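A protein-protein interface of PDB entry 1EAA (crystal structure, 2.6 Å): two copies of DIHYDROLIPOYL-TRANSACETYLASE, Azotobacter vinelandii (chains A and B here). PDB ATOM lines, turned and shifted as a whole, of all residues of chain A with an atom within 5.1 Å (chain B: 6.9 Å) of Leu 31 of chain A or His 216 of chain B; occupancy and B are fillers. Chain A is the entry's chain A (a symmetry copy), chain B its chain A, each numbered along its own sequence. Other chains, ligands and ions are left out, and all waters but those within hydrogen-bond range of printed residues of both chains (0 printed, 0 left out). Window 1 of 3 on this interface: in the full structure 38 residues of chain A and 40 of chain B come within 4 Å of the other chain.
A ring nitrogen (ND1) of His 40 of chain B is in hydrogen-bond range of the backbone carbonyl oxygen (O) of Val 38 of chain B, at 2.9 Å. N of His 216 of chain B lies within hydrogen-bond range of O of Pro 39 of chain B. O of Val 41 of chain B lies within hydrogen-bond range of N of Tyr 214 of chain B. The guanidinium group (NH2) of Arg 217 of chain B is in salt-bridge range of the side-chain carboxylate (OD2) of Asp 215 of chain B (2.8 Å). A ring nitrogen (ND1) of His 216 of chain B is in hydrogen-bond range of the backbone carbonyl oxygen (O) of Ile 219 of chain B, 3.1 Å away.
Among the printed residues, pairs that only touch across the chains: Ala 28 of chain A with Arg 217 of chain B (3.9 Å), Leu 31 of chain A with Pro 39 of chain B (3.8 Å), Leu 31 of chain A with His 216 of chain B (3.9 Å), Trp 35 of chain A with Val 38 of chain B (3.6 Å), Trp 35 of chain A with Pro 39 of chain B (3.7 Å), Trp 35 of chain A with His 40 of chain B (3.6 Å), Ile 177 of chain A with Pro 39 of chain B (3.7 Å), Ile 177 of chain A with His 40 of chain B (3.7 Å) and Ile 177 of chain A with Val 41 of chain B (3.9 Å).
Gly 27 of chain A touches none of the printed residues of chain B. Printed residues of chain B within 4 Å of Ala 28 of chain A: Arg 217 (3.9 Å). Printed residues of chain B within 4 Å of Ile 177 of chain A: Pro 39 (3.7 Å), His 40 (3.7 Å) and Val 41 (3.9 Å). Printed residues of chain A within 4 Å of Val 41 of chain B: Ile 177. Of chain A, only Leu 31 comes within 4 Å of His 216 of chain B. The nearest residue of chain B that does not touch Leu 31 of chain A is Arg 217 of chain B (4.6 Å). The nearest residue of chain A that does not touch His 216 of chain B is Ile 177 of chain A (4.2 Å). The nearest printed residue of chain A that does not touch Val 38 of chain B is His 32 of chain A (4.6 Å).
Of the 14 printed residues of chain B, 6 touch a printed residue of chain A. Printed residues of chain B that touch a printed residue of chain A: Val 38, Pro 39, His 40, Val 41, His 216 and Arg 217. Hydrophobic or aromatic side chains of chain B that line the printed part of chain A: Pro 39, His 40, Val 41 and His 216. Among the printed residues, 9 pairs touch across the chains. Among the printed residues, no Asp or Glu carboxylate lies within 4 Å of a Lys or Arg side-chain nitrogen of the other chain.
No position is printed for both chains. Of the 9 pairs that touch across the chains among the printed residues, none has its exchanged pair printed and touching as well.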
ATOM      1  N   ILE A  26      -5.719  -4.851  18.658  1.00  0.00           N
ATOM      2  CA  ILE A  26      -5.300  -4.819  17.275  1.00  0.00           C
ATOM      3  C   ILE A  26      -6.527  -5.220  16.494  1.00  0.00           C
ATOM      4  O   ILE A  26      -6.956  -4.486  15.609  1.00  0.00           O
ATOM      5  CB  ILE A  26      -4.176  -5.835  16.998  1.00  0.00           C
ATOM      6  CG1 ILE A  26      -2.884  -5.471  17.675  1.00  0.00           C
ATOM      7  CG2 ILE A  26      -3.901  -5.849  15.513  1.00  0.00           C
ATOM      8  CD1 ILE A  26      -2.392  -4.099  17.166  1.00  0.00           C
ATOM      9  N   GLY A  27      -7.104  -6.367  16.853  1.00  0.00           N
ATOM     10  CA  GLY A  27      -8.294  -6.905  16.232  1.00  0.00           C
ATOM     11  C   GLY A  27      -9.353  -5.833  16.136  1.00  0.00           C
ATOM     12  O   GLY A  27      -9.774  -5.485  15.030  1.00  0.00           O
ATOM     13  N   ALA A  28      -9.610  -5.175  17.259  1.00  0.00           N
ATOM     14  CA  ALA A  28     -10.639  -4.177  17.381  1.00  0.00           C
ATOM     15  C   ALA A  28     -10.429  -3.068  16.389  1.00  0.00           C
ATOM     16  O   ALA A  28     -11.352  -2.704  15.651  1.00  0.00           O
ATOM     17  CB  ALA A  28     -10.613  -3.583  18.758  1.00  0.00           C
ATOM     18  N   THR A  29      -9.202  -2.571  16.289  1.00  0.00           N
ATOM     19  CA  THR A  29      -8.921  -1.461  15.407  1.00  0.00           C
ATOM     20  C   THR A  29      -9.054  -1.785  13.934  1.00  0.00           C
ATOM     21  O   THR A  29      -9.643  -1.000  13.166  1.00  0.00           O
ATOM     22  CB  THR A  29      -7.528  -0.970  15.769  1.00  0.00           C
ATOM     23  OG1 THR A  29      -7.532  -0.673  17.175  1.00  0.00           O
ATOM     24  CG2 THR A  29      -7.167   0.274  14.998  1.00  0.00           C
ATOM     25  N   ASN A  30      -8.579  -2.967  13.565  1.00  0.00           N
ATOM     26  CA  ASN A  30      -8.675  -3.384  12.193  1.00  0.00           C
ATOM     27  C   ASN A  30     -10.109  -3.538  11.780  1.00  0.00           C
ATOM     28  O   ASN A  30     -10.461  -3.043  10.701  1.00  0.00           O
ATOM     29  CB  ASN A  30      -7.952  -4.694  11.962  1.00  0.00           C
ATOM     30  CG  ASN A  30      -6.457  -4.381  11.934  1.00  0.00           C
ATOM     31  OD1 ASN A  30      -5.916  -3.580  11.158  1.00  0.00           O
ATOM     32  ND2 ASN A  30      -5.701  -4.920  12.872  1.00  0.00           N
ATOM     33  N   LEU A  31     -11.000  -4.079  12.644  1.00  0.00           N
ATOM     34  CA  LEU A  31     -12.400  -4.221  12.257  1.00  0.00           C
ATOM     35  C   LEU A  31     -13.125  -2.914  12.112  1.00  0.00           C
ATOM     36  O   LEU A  31     -13.931  -2.749  11.194  1.00  0.00           O
ATOM     37  CB  LEU A  31     -13.147  -5.074  13.245  1.00  0.00           C
ATOM     38  CG  LEU A  31     -12.578  -6.459  13.243  1.00  0.00           C
ATOM     39  CD1 LEU A  31     -12.990  -7.108  14.515  1.00  0.00           C
ATOM     40  CD2 LEU A  31     -13.006  -7.223  12.014  1.00  0.00           C
ATOM     41  N   HIS A  32     -12.824  -1.963  12.973  1.00  0.00           N
ATOM     42  CA  HIS A  32     -13.466  -0.678  12.871  1.00  0.00           C
ATOM     43  C   HIS A  32     -12.941   0.037  11.635  1.00  0.00           C
ATOM     44  O   HIS A  32     -13.723   0.712  10.959  1.00  0.00           O
ATOM     45  CB  HIS A  32     -13.183   0.123  14.121  1.00  0.00           C
ATOM     46  CG  HIS A  32     -14.120   1.307  14.323  1.00  0.00           C
ATOM     47  ND1 HIS A  32     -13.923   2.380  15.080  1.00  0.00           N
ATOM     48  CD2 HIS A  32     -15.343   1.487  13.723  1.00  0.00           C
ATOM     49  CE1 HIS A  32     -14.951   3.188  14.949  1.00  0.00           C
ATOM     50  NE2 HIS A  32     -15.806   2.638  14.131  1.00  0.00           N
ATOM     51  N   ARG A  33     -11.662  -0.094  11.287  1.00  0.00           N
ATOM     52  CA  ARG A  33     -11.124   0.478  10.057  1.00  0.00           C
ATOM     53  C   ARG A  33     -11.822  -0.201   8.851  1.00  0.00           C
ATOM     54  O   ARG A  33     -12.150   0.521   7.904  1.00  0.00           O
ATOM     55  CB  ARG A  33      -9.622   0.240  10.121  1.00  0.00           C
ATOM     56  CG  ARG A  33      -8.702   1.004   9.213  1.00  0.00           C
ATOM     57  CD  ARG A  33      -7.767  -0.051   8.603  1.00  0.00           C
ATOM     58  NE  ARG A  33      -6.949  -0.796   9.553  1.00  0.00           N
ATOM     59  CZ  ARG A  33      -5.950  -0.197  10.221  1.00  0.00           C
ATOM     60  NH1 ARG A  33      -5.656   1.108  10.041  1.00  0.00           N
ATOM     61  NH2 ARG A  33      -5.270  -0.890  11.143  1.00  0.00           N
ATOM     62  N   SER A  34     -12.130  -1.524   8.837  1.00  0.00           N
ATOM     63  CA  SER A  34     -12.849  -2.196   7.760  1.00  0.00           C
ATOM     64  C   SER A  34     -14.256  -1.714   7.622  1.00  0.00           C
ATOM     65  O   SER A  34     -14.703  -1.396   6.529  1.00  0.00           O
ATOM     66  CB  SER A  34     -12.980  -3.683   7.951  1.00  0.00           C
ATOM     67  OG  SER A  34     -11.732  -4.346   7.813  1.00  0.00           O
ATOM     68  N   TRP A  35     -14.974  -1.675   8.737  1.00  0.00           N
ATOM     69  CA  TRP A  35     -16.355  -1.246   8.850  1.00  0.00           C
ATOM     70  C   TRP A  35     -16.636   0.154   8.310  1.00  0.00           C
ATOM     71  O   TRP A  35     -17.625   0.299   7.582  1.00  0.00           O
ATOM     72  CB  TRP A  35     -16.727  -1.306  10.301  1.00  0.00           C
ATOM     73  CG  TRP A  35     -18.146  -0.878  10.611  1.00  0.00           C
ATOM     74  CD1 TRP A  35     -18.483   0.318  11.201  1.00  0.00           C
ATOM     75  CD2 TRP A  35     -19.242  -1.639  10.334  1.00  0.00           C
ATOM     76  NE1 TRP A  35     -19.806   0.301  11.272  1.00  0.00           N
ATOM     77  CE2 TRP A  35     -20.285  -0.833  10.763  1.00  0.00           C
ATOM     78  CE3 TRP A  35     -19.428  -2.874   9.760  1.00  0.00           C
ATOM     79  CZ2 TRP A  35     -21.568  -1.268  10.632  1.00  0.00           C
ATOM     80  CZ3 TRP A  35     -20.707  -3.299   9.632  1.00  0.00           C
ATOM     81  CH2 TRP A  35     -21.752  -2.507  10.069  1.00  0.00           C
ATOM     82  N   LEU A  36     -15.815   1.177   8.655  1.00  0.00           N
ATOM     83  CA  LEU A  36     -16.049   2.548   8.197  1.00  0.00           C
ATOM     84  C   LEU A  36     -15.624   2.748   6.764  1.00  0.00           C
ATOM     85  O   LEU A  36     -16.118   3.630   6.061  1.00  0.00           O
ATOM     86  CB  LEU A  36     -15.294   3.518   9.052  1.00  0.00           C
ATOM     87  CG  LEU A  36     -15.823   3.590  10.459  1.00  0.00           C
ATOM     88  CD1 LEU A  36     -14.890   4.412  11.295  1.00  0.00           C
ATOM     89  CD2 LEU A  36     -17.187   4.196  10.466  1.00  0.00           C
ATOM     90  N   ILE A 177     -17.419  -9.543   8.678  1.00  0.00           N
ATOM     91  CA  ILE A 177     -16.847  -8.273   8.224  1.00  0.00           C
ATOM     92  C   ILE A 177     -15.632  -8.563   7.335  1.00  0.00           C
ATOM     93  O   ILE A 177     -14.854  -9.464   7.569  1.00  0.00           O
ATOM     94  CB  ILE A 177     -16.464  -7.419   9.462  1.00  0.00           C
ATOM     95  CG1 ILE A 177     -17.758  -6.930  10.075  1.00  0.00           C
ATOM     96  CG2 ILE A 177     -15.513  -6.301   9.101  1.00  0.00           C
ATOM     97  CD1 ILE A 177     -17.545  -6.052  11.275  1.00  0.00           C
ATOM     98  N   ASN A 179     -12.084  -8.252   5.734  1.00  0.00           N
ATOM     99  CA  ASN A 179     -10.748  -7.887   6.177  1.00  0.00           C
ATOM    100  C   ASN A 179     -10.090  -7.084   5.058  1.00  0.00           C
ATOM    101  O   ASN A 179      -9.377  -7.605   4.180  1.00  0.00           O
ATOM    102  CB  ASN A 179      -9.879  -9.099   6.438  1.00  0.00           C
ATOM    103  CG  ASN A 179     -10.383 -10.009   7.554  1.00  0.00           C
ATOM    104  OD1 ASN A 179     -10.576  -9.664   8.728  1.00  0.00           O
ATOM    105  ND2 ASN A 179     -10.620 -11.249   7.141  1.00  0.00           N
ATOM    106  N   VAL B  38     -19.656   1.102  16.108  1.00  0.00           N
ATOM    107  CA  VAL B  38     -19.643  -0.297  16.432  1.00  0.00           C
ATOM    108  C   VAL B  38     -19.477  -1.186  15.204  1.00  0.00           C
ATOM    109  O   VAL B  38     -20.437  -1.260  14.431  1.00  0.00           O
ATOM    110  CB  VAL B  38     -20.951  -0.547  17.163  1.00  0.00           C
ATOM    111  CG1 VAL B  38     -20.958  -1.948  17.657  1.00  0.00           C
ATOM    112  CG2 VAL B  38     -21.097   0.331  18.352  1.00  0.00           C
ATOM    113  N   PRO B  39     -18.413  -1.929  14.907  1.00  0.00           N
ATOM    114  CA  PRO B  39     -18.403  -2.814  13.749  1.00  0.00           C
ATOM    115  C   PRO B  39     -19.316  -3.985  14.065  1.00  0.00           C
ATOM    116  O   PRO B  39     -19.011  -4.822  14.918  1.00  0.00           O
ATOM    117  CB  PRO B  39     -16.933  -3.151  13.542  1.00  0.00           C
ATOM    118  CG  PRO B  39     -16.373  -3.001  14.903  1.00  0.00           C
ATOM    119  CD  PRO B  39     -17.129  -1.845  15.561  1.00  0.00           C
ATOM    120  N   HIS B  40     -20.491  -3.961  13.423  1.00  0.00           N
ATOM    121  CA  HIS B  40     -21.570  -4.933  13.642  1.00  0.00           C
ATOM    122  C   HIS B  40     -21.505  -6.233  12.884  1.00  0.00           C
ATOM    123  O   HIS B  40     -21.164  -6.274  11.695  1.00  0.00           O
ATOM    124  CB  HIS B  40     -22.947  -4.365  13.295  1.00  0.00           C
ATOM    125  CG  HIS B  40     -23.505  -3.202  14.137  1.00  0.00           C
ATOM    126  ND1 HIS B  40     -23.188  -1.911  14.039  1.00  0.00           N
ATOM    127  CD2 HIS B  40     -24.482  -3.299  15.123  1.00  0.00           C
ATOM    128  CE1 HIS B  40     -23.920  -1.238  14.882  1.00  0.00           C
ATOM    129  NE2 HIS B  40     -24.692  -2.065  15.529  1.00  0.00           N
ATOM    130  N   VAL B  41     -21.871  -7.308  13.538  1.00  0.00           N
ATOM    131  CA  VAL B  41     -22.060  -8.571  12.850  1.00  0.00           C
ATOM    132  C   VAL B  41     -23.395  -9.081  13.381  1.00  0.00           C
ATOM    133  O   VAL B  41     -23.730  -8.771  14.524  1.00  0.00           O
ATOM    134  CB  VAL B  41     -20.946  -9.599  13.175  1.00  0.00           C
ATOM    135  CG1 VAL B  41     -21.170 -10.899  12.413  1.00  0.00           C
ATOM    136  CG2 VAL B  41     -19.614  -9.087  12.708  1.00  0.00           C
ATOM    137  N   VAL B 183     -23.112  -4.022  24.276  1.00  0.00           N
ATOM    138  CA  VAL B 183     -22.309  -4.751  23.316  1.00  0.00           C
ATOM    139  C   VAL B 183     -23.066  -5.775  22.454  1.00  0.00           C
ATOM    140  O   VAL B 183     -22.463  -6.316  21.520  1.00  0.00           O
ATOM    141  CB  VAL B 183     -21.219  -5.225  24.286  1.00  0.00           C
ATOM    142  CG1 VAL B 183     -21.056  -6.674  24.310  1.00  0.00           C
ATOM    143  CG2 VAL B 183     -19.945  -4.538  23.905  1.00  0.00           C
ATOM    144  N   TYR B 214     -23.817  -8.051  17.438  1.00  0.00           N
ATOM    145  CA  TYR B 214     -22.870  -7.765  18.497  1.00  0.00           C
ATOM    146  C   TYR B 214     -21.806  -6.792  18.115  1.00  0.00           C
ATOM    147  O   TYR B 214     -21.698  -6.450  16.939  1.00  0.00           O
ATOM    148  CB  TYR B 214     -22.177  -8.978  18.961  1.00  0.00           C
ATOM    149  CG  TYR B 214     -21.622  -9.883  17.906  1.00  0.00           C
ATOM    150  CD1 TYR B 214     -22.452 -10.768  17.277  1.00  0.00           C
ATOM    151  CD2 TYR B 214     -20.271  -9.882  17.615  1.00  0.00           C
ATOM    152  CE1 TYR B 214     -21.906 -11.665  16.367  1.00  0.00           C
ATOM    153  CE2 TYR B 214     -19.723 -10.784  16.703  1.00  0.00           C
ATOM    154  CZ  TYR B 214     -20.546 -11.682  16.076  1.00  0.00           C
ATOM    155  OH  TYR B 214     -20.029 -12.591  15.159  1.00  0.00           O
ATOM    156  N   ASP B 215     -21.035  -6.299  19.077  1.00  0.00           N
ATOM    157  CA  ASP B 215     -19.956  -5.392  18.748  1.00  0.00           C
ATOM    158  C   ASP B 215     -18.747  -6.283  18.510  1.00  0.00           C
ATOM    159  O   ASP B 215     -18.077  -6.725  19.458  1.00  0.00           O
ATOM    160  CB  ASP B 215     -19.674  -4.477  19.894  1.00  0.00           C
ATOM    161  CG  ASP B 215     -18.550  -3.475  19.684  1.00  0.00           C
ATOM    162  OD1 ASP B 215     -17.688  -3.615  18.802  1.00  0.00           O
ATOM    163  OD2 ASP B 215     -18.570  -2.520  20.447  1.00  0.00           O
ATOM    164  N   HIS B 216     -18.379  -6.446  17.238  1.00  0.00           N
ATOM    165  CA  HIS B 216     -17.326  -7.384  16.921  1.00  0.00           C
ATOM    166  C   HIS B 216     -16.010  -7.024  17.599  1.00  0.00           C
ATOM    167  O   HIS B 216     -15.208  -7.934  17.766  1.00  0.00           O
ATOM    168  CB  HIS B 216     -17.131  -7.455  15.413  1.00  0.00           C
ATOM    169  CG  HIS B 216     -16.500  -8.786  14.990  1.00  0.00           C
ATOM    170  ND1 HIS B 216     -15.999  -9.762  15.750  1.00  0.00           N
ATOM    171  CD2 HIS B 216     -16.350  -9.224  13.694  1.00  0.00           C
ATOM    172  CE1 HIS B 216     -15.576 -10.736  14.990  1.00  0.00           C
ATOM    173  NE2 HIS B 216     -15.789 -10.408  13.750  1.00  0.00           N
ATOM    174  N   ARG B 217     -15.730  -5.769  18.021  1.00  0.00           N
ATOM    175  CA  ARG B 217     -14.529  -5.408  18.772  1.00  0.00           C
ATOM    176  C   ARG B 217     -14.363  -6.181  20.086  1.00  0.00           C
ATOM    177  O   ARG B 217     -13.282  -6.517  20.538  1.00  0.00           O
ATOM    178  CB  ARG B 217     -14.546  -3.939  19.156  1.00  0.00           C
ATOM    179  CG  ARG B 217     -14.526  -2.980  17.985  1.00  0.00           C
ATOM    180  CD  ARG B 217     -14.719  -1.548  18.413  1.00  0.00           C
ATOM    181  NE  ARG B 217     -15.922  -1.396  19.209  1.00  0.00           N
ATOM    182  CZ  ARG B 217     -16.332  -0.199  19.600  1.00  0.00           C
ATOM    183  NH1 ARG B 217     -15.643   0.886  19.249  1.00  0.00           N
ATOM    184  NH2 ARG B 217     -17.357  -0.046  20.435  1.00  0.00           N
ATOM    185  N   VAL B 218     -15.472  -6.398  20.765  1.00  0.00           N
ATOM    186  CA  VAL B 218     -15.518  -7.051  22.054  1.00  0.00           C
ATOM    187  C   VAL B 218     -15.872  -8.535  21.869  1.00  0.00           C
ATOM    188  O   VAL B 218     -15.189  -9.367  22.477  1.00  0.00           O
ATOM    189  CB  VAL B 218     -16.570  -6.335  22.903  1.00  0.00           C
ATOM    190  CG1 VAL B 218     -16.732  -7.019  24.244  1.00  0.00           C
ATOM    191  CG2 VAL B 218     -16.156  -4.880  23.065  1.00  0.00           C
ATOM    192  N   ILE B 219     -16.888  -8.927  21.064  1.00  0.00           N
ATOM    193  CA  ILE B 219     -17.277 -10.319  20.963  1.00  0.00           C
ATOM    194  C   ILE B 219     -16.852 -10.854  19.647  1.00  0.00           C
ATOM    195  O   ILE B 219     -17.120 -10.261  18.607  1.00  0.00           O
ATOM    196  CB  ILE B 219     -18.807 -10.447  21.129  1.00  0.00           C
ATOM    197  CG1 ILE B 219     -19.024 -10.495  22.600  1.00  0.00           C
ATOM    198  CG2 ILE B 219     -19.434 -11.724  20.596  1.00  0.00           C
ATOM    199  CD1 ILE B 219     -19.772  -9.260  22.893  1.00  0.00           C
ATOM    200  N   ASN B 220     -16.175 -11.962  19.622  1.00  0.00           N
ATOM    201  CA  ASN B 220     -15.825 -12.594  18.350  1.00  0.00           C
ATOM    202  C   ASN B 220     -16.931 -13.517  17.900  1.00  0.00           C
ATOM    203  O   ASN B 220     -17.823 -13.887  18.665  1.00  0.00           O
ATOM    204  CB  ASN B 220     -14.546 -13.431  18.434  1.00  0.00           C
ATOM    205  CG  ASN B 220     -14.565 -14.370  19.630  1.00  0.00           C
ATOM    206  OD1 ASN B 220     -14.813 -13.954  20.761  1.00  0.00           O
ATOM    207  ND2 ASN B 220     -14.358 -15.674  19.581  1.00  0.00           N
ATOM    208  N   GLY B 221     -16.807 -13.959  16.657  1.00  0.00           N
ATOM    209  CA  GLY B 221     -17.757 -14.840  16.029  1.00  0.00           C
ATOM    210  C   GLY B 221     -18.000 -16.123  16.782  1.00  0.00           C
ATOM    211  O   GLY B 221     -19.154 -16.488  17.019  1.00  0.00           O
ATOM    212  N   ALA B 222     -16.988 -16.844  17.215  1.00  0.00           N
ATOM    213  CA  ALA B 222     -17.265 -18.033  17.986  1.00  0.00           C
ATOM    214  C   ALA B 222     -17.943 -17.737  19.317  1.00  0.00           C
ATOM    215  O   ALA B 222     -18.798 -18.507  19.725  1.00  0.00           O
ATOM    216  CB  ALA B 222     -16.019 -18.723  18.251  1.00  0.00           C
